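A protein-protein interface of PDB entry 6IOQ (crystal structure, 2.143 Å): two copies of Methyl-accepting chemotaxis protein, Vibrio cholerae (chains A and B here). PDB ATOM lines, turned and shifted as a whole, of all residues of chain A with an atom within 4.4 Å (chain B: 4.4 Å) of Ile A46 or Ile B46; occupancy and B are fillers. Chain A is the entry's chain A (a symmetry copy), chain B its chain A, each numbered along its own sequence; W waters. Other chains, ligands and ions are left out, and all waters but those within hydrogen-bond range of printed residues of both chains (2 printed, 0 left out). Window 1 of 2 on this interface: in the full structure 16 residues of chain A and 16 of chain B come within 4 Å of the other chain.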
ATOM      1  N   SER A  42     -22.678   8.514  17.539  1.00  0.00           N
ATOM      2  CA  SER A  42     -22.299   9.912  17.740  1.00  0.00           C
ATOM      3  C   SER A  42     -21.378  10.448  16.666  1.00  0.00           C
ATOM      4  O   SER A  42     -21.498  11.616  16.298  1.00  0.00           O
ATOM      5  CB  SER A  42     -21.635  10.116  19.096  1.00  0.00           C
ATOM      6  OG  SER A  42     -22.617  10.171  20.118  1.00  0.00           O
ATOM      7  N   THR A  43     -20.446   9.626  16.173  1.00  0.00           N
ATOM      8  CA  THR A  43     -19.508  10.100  15.157  1.00  0.00           C
ATOM      9  C   THR A  43     -20.255  10.419  13.884  1.00  0.00           C
ATOM     10  O   THR A  43     -20.021  11.443  13.244  1.00  0.00           O
ATOM     11  CB  THR A  43     -18.419   9.077  14.834  1.00  0.00           C
ATOM     12  OG1 THR A  43     -17.645   8.810  16.001  1.00  0.00           O
ATOM     13  CG2 THR A  43     -17.495   9.617  13.753  1.00  0.00           C
ATOM     14  N   THR A  44     -21.176   9.539  13.524  1.00  0.00           N
ATOM     15  CA  THR A  44     -21.992   9.750  12.342  1.00  0.00           C
ATOM     16  C   THR A  44     -22.833  11.038  12.458  1.00  0.00           C
ATOM     17  O   THR A  44     -22.900  11.849  11.523  1.00  0.00           O
ATOM     18  CB  THR A  44     -22.912   8.558  12.112  1.00  0.00           C
ATOM     19  OG1 THR A  44     -22.120   7.361  12.047  1.00  0.00           O
ATOM     20  CG2 THR A  44     -23.690   8.742  10.826  1.00  0.00           C
ATOM     21  N   GLU A  45     -23.455  11.230  13.617  1.00  0.00           N
ATOM     22  CA  GLU A  45     -24.296  12.409  13.838  1.00  0.00           C
ATOM     23  C   GLU A  45     -23.468  13.664  13.769  1.00  0.00           C
ATOM     24  O   GLU A  45     -23.909  14.676  13.218  1.00  0.00           O
ATOM     25  CB  GLU A  45     -25.023  12.323  15.185  1.00  0.00           C
ATOM     26  CG  GLU A  45     -26.106  11.278  15.157  1.00  0.00           C
ATOM     27  CD  GLU A  45     -26.748  11.037  16.490  1.00  0.00           C
ATOM     28  OE1 GLU A  45     -26.311  11.635  17.502  1.00  0.00           O
ATOM     29  OE2 GLU A  45     -27.699  10.229  16.525  1.00  0.00           O
ATOM     30  N   ILE A  46     -22.256  13.604  14.305  1.00  0.00           N
ATOM     31  CA  ILE A  46     -21.394  14.773  14.264  1.00  0.00           C
ATOM     32  C   ILE A  46     -20.967  15.078  12.822  1.00  0.00           C
ATOM     33  O   ILE A  46     -21.035  16.227  12.389  1.00  0.00           O
ATOM     34  CB  ILE A  46     -20.171  14.603  15.181  1.00  0.00           C
ATOM     35  CG1 ILE A  46     -20.623  14.739  16.644  1.00  0.00           C
ATOM     36  CG2 ILE A  46     -19.095  15.627  14.843  1.00  0.00           C
ATOM     37  CD1 ILE A  46     -19.555  14.468  17.673  1.00  0.00           C
ATOM     38  N   LEU A  47     -20.579  14.056  12.066  1.00  0.00           N
ATOM     39  CA  LEU A  47     -20.246  14.252  10.658  1.00  0.00           C
ATOM     40  C   LEU A  47     -21.427  14.787   9.850  1.00  0.00           C
ATOM     41  O   LEU A  47     -21.224  15.456   8.843  1.00  0.00           O
ATOM     42  CB  LEU A  47     -19.757  12.949  10.028  1.00  0.00           C
ATOM     43  CG  LEU A  47     -18.318  12.575  10.414  1.00  0.00           C
ATOM     44  CD1 LEU A  47     -17.793  11.453   9.555  1.00  0.00           C
ATOM     45  CD2 LEU A  47     -17.422  13.787  10.303  1.00  0.00           C
ATOM     46  N   GLN A  48     -22.654  14.487  10.292  1.00  0.00           N
ATOM     47  CA  GLN A  48     -23.859  14.976   9.614  1.00  0.00           C
ATOM     48  C   GLN A  48     -24.100  16.475   9.786  1.00  0.00           C
ATOM     49  O   GLN A  48     -25.014  17.024   9.186  1.00  0.00           O
ATOM     50  CB  GLN A  48     -25.085  14.200  10.079  1.00  0.00           C
ATOM     51  CG  GLN A  48     -25.188  12.862   9.376  1.00  0.00           C
ATOM     52  CD  GLN A  48     -26.436  12.106   9.716  1.00  0.00           C
ATOM     53  OE1 GLN A  48     -26.720  11.062   9.127  1.00  0.00           O
ATOM     54  NE2 GLN A  48     -27.206  12.629  10.668  1.00  0.00           N
ATOM     55  N   LEU A  49     -23.277  17.133  10.589  1.00  0.00           N
ATOM     56  CA  LEU A  49     -23.285  18.592  10.662  1.00  0.00           C
ATOM     57  C   LEU A  49     -22.736  19.207   9.363  1.00  0.00           C
ATOM     58  O   LEU A  49     -23.066  20.338   9.018  1.00  0.00           O
ATOM     59  CB  LEU A  49     -22.460  19.072  11.857  1.00  0.00           C
ATOM     60  CG  LEU A  49     -22.957  18.636  13.238  1.00  0.00           C
ATOM     61  CD1 LEU A  49     -21.965  19.065  14.314  1.00  0.00           C
ATOM     62  CD2 LEU A  49     -24.338  19.177  13.514  1.00  0.00           C
ATOM     63  N   PHE A  56     -13.163  18.059   7.083  1.00  0.00           N
ATOM     64  CA  PHE A  56     -13.736  17.927   8.425  1.00  0.00           C
ATOM     65  C   PHE A  56     -13.887  16.454   8.780  1.00  0.00           C
ATOM     66  O   PHE A  56     -13.565  16.019   9.886  1.00  0.00           O
ATOM     67  CB  PHE A  56     -15.084  18.640   8.484  1.00  0.00           C
ATOM     68  CG  PHE A  56     -15.895  18.360   9.730  1.00  0.00           C
ATOM     69  CD1 PHE A  56     -15.384  18.630  10.985  1.00  0.00           C
ATOM     70  CD2 PHE A  56     -17.196  17.896   9.633  1.00  0.00           C
ATOM     71  CE1 PHE A  56     -16.144  18.401  12.135  1.00  0.00           C
ATOM     72  CE2 PHE A  56     -17.955  17.669  10.775  1.00  0.00           C
ATOM     73  CZ  PHE A  56     -17.419  17.921  12.026  1.00  0.00           C
ATOM     74  N   VAL A  60     -12.091  14.308  11.908  1.00  0.00           N
ATOM     75  CA  VAL A  60     -12.842  13.565  12.909  1.00  0.00           C
ATOM     76  C   VAL A  60     -12.340  12.119  13.000  1.00  0.00           C
ATOM     77  O   VAL A  60     -12.055  11.620  14.088  1.00  0.00           O
ATOM     78  CB  VAL A  60     -14.345  13.587  12.575  1.00  0.00           C
ATOM     79  CG1 VAL A  60     -15.080  12.536  13.359  1.00  0.00           C
ATOM     80  CG2 VAL A  60     -14.915  14.977  12.864  1.00  0.00           C
ATOM     81  N   SER A  63      -9.041  11.661  14.749  1.00  0.00           N
ATOM     82  CA  SER A  63      -8.929  12.005  16.168  1.00  0.00           C
ATOM     83  C   SER A  63      -8.599  10.752  16.956  1.00  0.00           C
ATOM     84  O   SER A  63      -9.204   9.705  16.723  1.00  0.00           O
ATOM     85  CB  SER A  63     -10.224  12.644  16.696  1.00  0.00           C
ATOM     86  OG  SER A  63     -11.321  11.760  16.541  1.00  0.00           O
ATOM     87  N   SER B  42     -13.715  11.334  23.034  1.00  0.00           N
ATOM     88  CA  SER B  42     -13.883  11.640  21.614  1.00  0.00           C
ATOM     89  C   SER B  42     -14.575  12.963  21.360  1.00  0.00           C
ATOM     90  O   SER B  42     -14.225  13.650  20.401  1.00  0.00           O
ATOM     91  CB  SER B  42     -14.658  10.541  20.899  1.00  0.00           C
ATOM     92  OG  SER B  42     -13.806   9.441  20.624  1.00  0.00           O
ATOM     93  N   THR B  43     -15.564  13.320  22.185  1.00  0.00           N
ATOM     94  CA  THR B  43     -16.288  14.571  21.967  1.00  0.00           C
ATOM     95  C   THR B  43     -15.356  15.742  22.176  1.00  0.00           C
ATOM     96  O   THR B  43     -15.346  16.696  21.401  1.00  0.00           O
ATOM     97  CB  THR B  43     -17.484  14.734  22.907  1.00  0.00           C
ATOM     98  OG1 THR B  43     -18.421  13.683  22.681  1.00  0.00           O
ATOM     99  CG2 THR B  43     -18.177  16.063  22.650  1.00  0.00           C
ATOM    100  N   THR B  44     -14.555  15.656  23.226  1.00  0.00           N
ATOM    101  CA  THR B  44     -13.584  16.697  23.513  1.00  0.00           C
ATOM    102  C   THR B  44     -12.565  16.850  22.366  1.00  0.00           C
ATOM    103  O   THR B  44     -12.259  17.967  21.923  1.00  0.00           O
ATOM    104  CB  THR B  44     -12.849  16.393  24.812  1.00  0.00           C
ATOM    105  OG1 THR B  44     -13.812  16.211  25.863  1.00  0.00           O
ATOM    106  CG2 THR B  44     -11.908  17.529  25.155  1.00  0.00           C
ATOM    107  N   GLU B  45     -12.058  15.724  21.875  1.00  0.00           N
ATOM    108  CA  GLU B  45     -11.068  15.746  20.796  1.00  0.00           C
ATOM    109  C   GLU B  45     -11.668  16.334  19.546  1.00  0.00           C
ATOM    110  O   GLU B  45     -11.008  17.092  18.832  1.00  0.00           O
ATOM    111  CB  GLU B  45     -10.527  14.340  20.516  1.00  0.00           C
ATOM    112  CG  GLU B  45      -9.632  13.866  21.629  1.00  0.00           C
ATOM    113  CD  GLU B  45      -9.197  12.439  21.490  1.00  0.00           C
ATOM    114  OE1 GLU B  45      -9.645  11.747  20.545  1.00  0.00           O
ATOM    115  OE2 GLU B  45      -8.399  12.000  22.346  1.00  0.00           O
ATOM    116  N   ILE B  46     -12.928  16.010  19.286  1.00  0.00           N
ATOM    117  CA  ILE B  46     -13.579  16.551  18.103  1.00  0.00           C
ATOM    118  C   ILE B  46     -13.780  18.066  18.245  1.00  0.00           C
ATOM    119  O   ILE B  46     -13.476  18.817  17.319  1.00  0.00           O
ATOM    120  CB  ILE B  46     -14.910  15.838  17.818  1.00  0.00           C
ATOM    121  CG1 ILE B  46     -14.615  14.436  17.261  1.00  0.00           C
ATOM    122  CG2 ILE B  46     -15.760  16.646  16.846  1.00  0.00           C
ATOM    123  CD1 ILE B  46     -15.826  13.561  17.051  1.00  0.00           C
ATOM    124  N   LEU B  47     -14.239  18.519  19.406  1.00  0.00           N
ATOM    125  CA  LEU B  47     -14.370  19.954  19.649  1.00  0.00           C
ATOM    126  C   LEU B  47     -13.031  20.685  19.552  1.00  0.00           C
ATOM    127  O   LEU B  47     -13.005  21.868  19.234  1.00  0.00           O
ATOM    128  CB  LEU B  47     -14.987  20.219  21.021  1.00  0.00           C
ATOM    129  CG  LEU B  47     -16.503  19.975  21.077  1.00  0.00           C
ATOM    130  CD1 LEU B  47     -17.100  20.517  22.351  1.00  0.00           C
ATOM    131  CD2 LEU B  47     -17.171  20.600  19.874  1.00  0.00           C
ATOM    132  N   GLN B  48     -11.929  19.979  19.829  1.00  0.00           N
ATOM    133  CA  GLN B  48     -10.591  20.570  19.734  1.00  0.00           C
ATOM    134  C   GLN B  48     -10.131  20.834  18.302  1.00  0.00           C
ATOM    135  O   GLN B  48      -9.077  21.418  18.092  1.00  0.00           O
ATOM    136  CB  GLN B  48      -9.569  19.695  20.450  1.00  0.00           C
ATOM    137  CG  GLN B  48      -9.603  19.921  21.948  1.00  0.00           C
ATOM    138  CD  GLN B  48      -8.542  19.166  22.688  1.00  0.00           C
ATOM    139  OE1 GLN B  48      -8.366  19.348  23.894  1.00  0.00           O
ATOM    140  NE2 GLN B  48      -7.814  18.312  21.973  1.00  0.00           N
ATOM    141  N   LEU B  49     -10.923  20.420  17.325  1.00  0.00           N
ATOM    142  CA  LEU B  49     -10.688  20.803  15.935  1.00  0.00           C
ATOM    143  C   LEU B  49     -10.975  22.299  15.723  1.00  0.00           C
ATOM    144  O   LEU B  49     -10.428  22.920  14.817  1.00  0.00           O
ATOM    145  CB  LEU B  49     -11.557  19.965  14.995  1.00  0.00           C
ATOM    146  CG  LEU B  49     -11.301  18.456  15.006  1.00  0.00           C
ATOM    147  CD1 LEU B  49     -12.329  17.742  14.133  1.00  0.00           C
ATOM    148  CD2 LEU B  49      -9.892  18.141  14.567  1.00  0.00           C
ATOM    149  N   PHE B  56     -20.277  25.632  16.442  1.00  0.00           N
ATOM    150  CA  PHE B  56     -19.894  24.241  16.189  1.00  0.00           C
ATOM    151  C   PHE B  56     -20.025  23.427  17.469  1.00  0.00           C
ATOM    152  O   PHE B  56     -20.540  22.308  17.474  1.00  0.00           O
ATOM    153  CB  PHE B  56     -18.463  24.188  15.658  1.00  0.00           C
ATOM    154  CG  PHE B  56     -17.859  22.803  15.603  1.00  0.00           C
ATOM    155  CD1 PHE B  56     -18.461  21.793  14.876  1.00  0.00           C
ATOM    156  CD2 PHE B  56     -16.648  22.539  16.220  1.00  0.00           C
ATOM    157  CE1 PHE B  56     -17.887  20.522  14.799  1.00  0.00           C
ATOM    158  CE2 PHE B  56     -16.074  21.275  16.144  1.00  0.00           C
ATOM    159  CZ  PHE B  56     -16.703  20.268  15.433  1.00  0.00           C
ATOM    160  N   VAL B  60     -22.496  20.123  18.238  1.00  0.00           N
ATOM    161  CA  VAL B  60     -21.998  18.833  18.690  1.00  0.00           C
ATOM    162  C   VAL B  60     -22.735  18.381  19.956  1.00  0.00           C
ATOM    163  O   VAL B  60     -23.221  17.253  20.032  1.00  0.00           O
ATOM    164  CB  VAL B  60     -20.482  18.909  18.955  1.00  0.00           C
ATOM    165  CG1 VAL B  60     -20.023  17.730  19.766  1.00  0.00           C
ATOM    166  CG2 VAL B  60     -19.732  18.976  17.623  1.00  0.00           C
ATOM    167  N   SER B  63     -26.245  17.136  19.426  1.00  0.00           N
ATOM    168  CA  SER B  63     -26.463  15.931  18.622  1.00  0.00           C
ATOM    169  C   SER B  63     -27.081  14.858  19.497  1.00  0.00           C
ATOM    170  O   SER B  63     -26.631  14.653  20.626  1.00  0.00           O
ATOM    171  CB  SER B  63     -25.152  15.425  17.999  1.00  0.00           C
ATOM    172  OG  SER B  63     -24.202  15.118  19.005  1.00  0.00           O
HETATM  173  O   HOH W   1     -11.542  10.847  19.093  1.00  0.00           O
HETATM  174  O   HOH W   2     -24.430  12.408  19.044  1.00  0.00           O
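The side-chain hydroxyl of Ser B63 sits at hydrogen-bond distance from the backbone carbonyl oxygen of Val B60 (2.6 Å). OG of Ser A63 is in hydrogen-bond range of O of Val A60 (2.6 Å).
Among the printed residues, merely in contact across the chains: Phe A56 with Phe B56 (3.8 Å), Glu A45 with Ser B63 (3.9 Å), Ser A63 with Glu B45 (3.9 Å), Ile A46 with Ile B46 (3.9 Å), Val A60 with Ile B46 (3.9 Å), Ile A46 with Val B60 (3.9 Å), Val A60 with Leu B49 (3.99 Å) and Leu A49 with Val B60 (3.99 Å).
Ile A46 touches just these residues of chain B: Ile B46 and Val B60. Ile B46 touches two residues of chain A. Of the printed residues of chain A, Glu B45 touches Ser A63. Of the printed residues of chain A, Val B60 touches Ile A46 (3.9 Å) and Leu A49 (3.99 Å). Thr A44 touches none of the printed residues of chain B. The nearest residue of chain B that does not touch Ile A46 is Ser B63 (4.3 Å).
Of the 11 printed residues of chain B, 6 touch a printed residue of chain A. Printed residues of chain B that touch a printed residue of chain A: Glu B45, Ile B46, Leu B49, Phe B56, Val B60 and Ser B63. Hydrophobic or aromatic side chains of chain B within 4 Å of the printed part of chain A: Ile B46, Leu B49, Phe B56 and Val B60. Of the 11 printed residues of chain A, 6 touch a printed residue of chain B. Hydrophobic or aromatic side chains of chain A that line the printed part of chain B: Ile A46, Leu A49, Phe A56 and Val A60. Among the printed residues, 8 pairs touch across the chains. Among the printed residues, no Asp or Glu carboxylate lies within 4 Å of a Lys or Arg side-chain nitrogen of the other chain.
Glu A45 touches Ser B63, and with the chains exchanged Ser A63 touches Glu B45. Ile A46 touches Val B60, and with the chains exchanged Val A60 touches Ile B46. Leu A49 touches Val B60, and with the chains exchanged Val A60 touches Leu B49. Phe A56 touches its own counterpart, Phe B56.
Water W1 lies within hydrogen-bond range of the side-chain carboxylate of Glu B45, the side-chain hydroxyl of Ser A63 and the side-chain hydroxyl of Ser B42. Water W2 lies within hydrogen-bond range of OE1 of Glu A45, OG of Ser B63 and OG of Ser A42.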
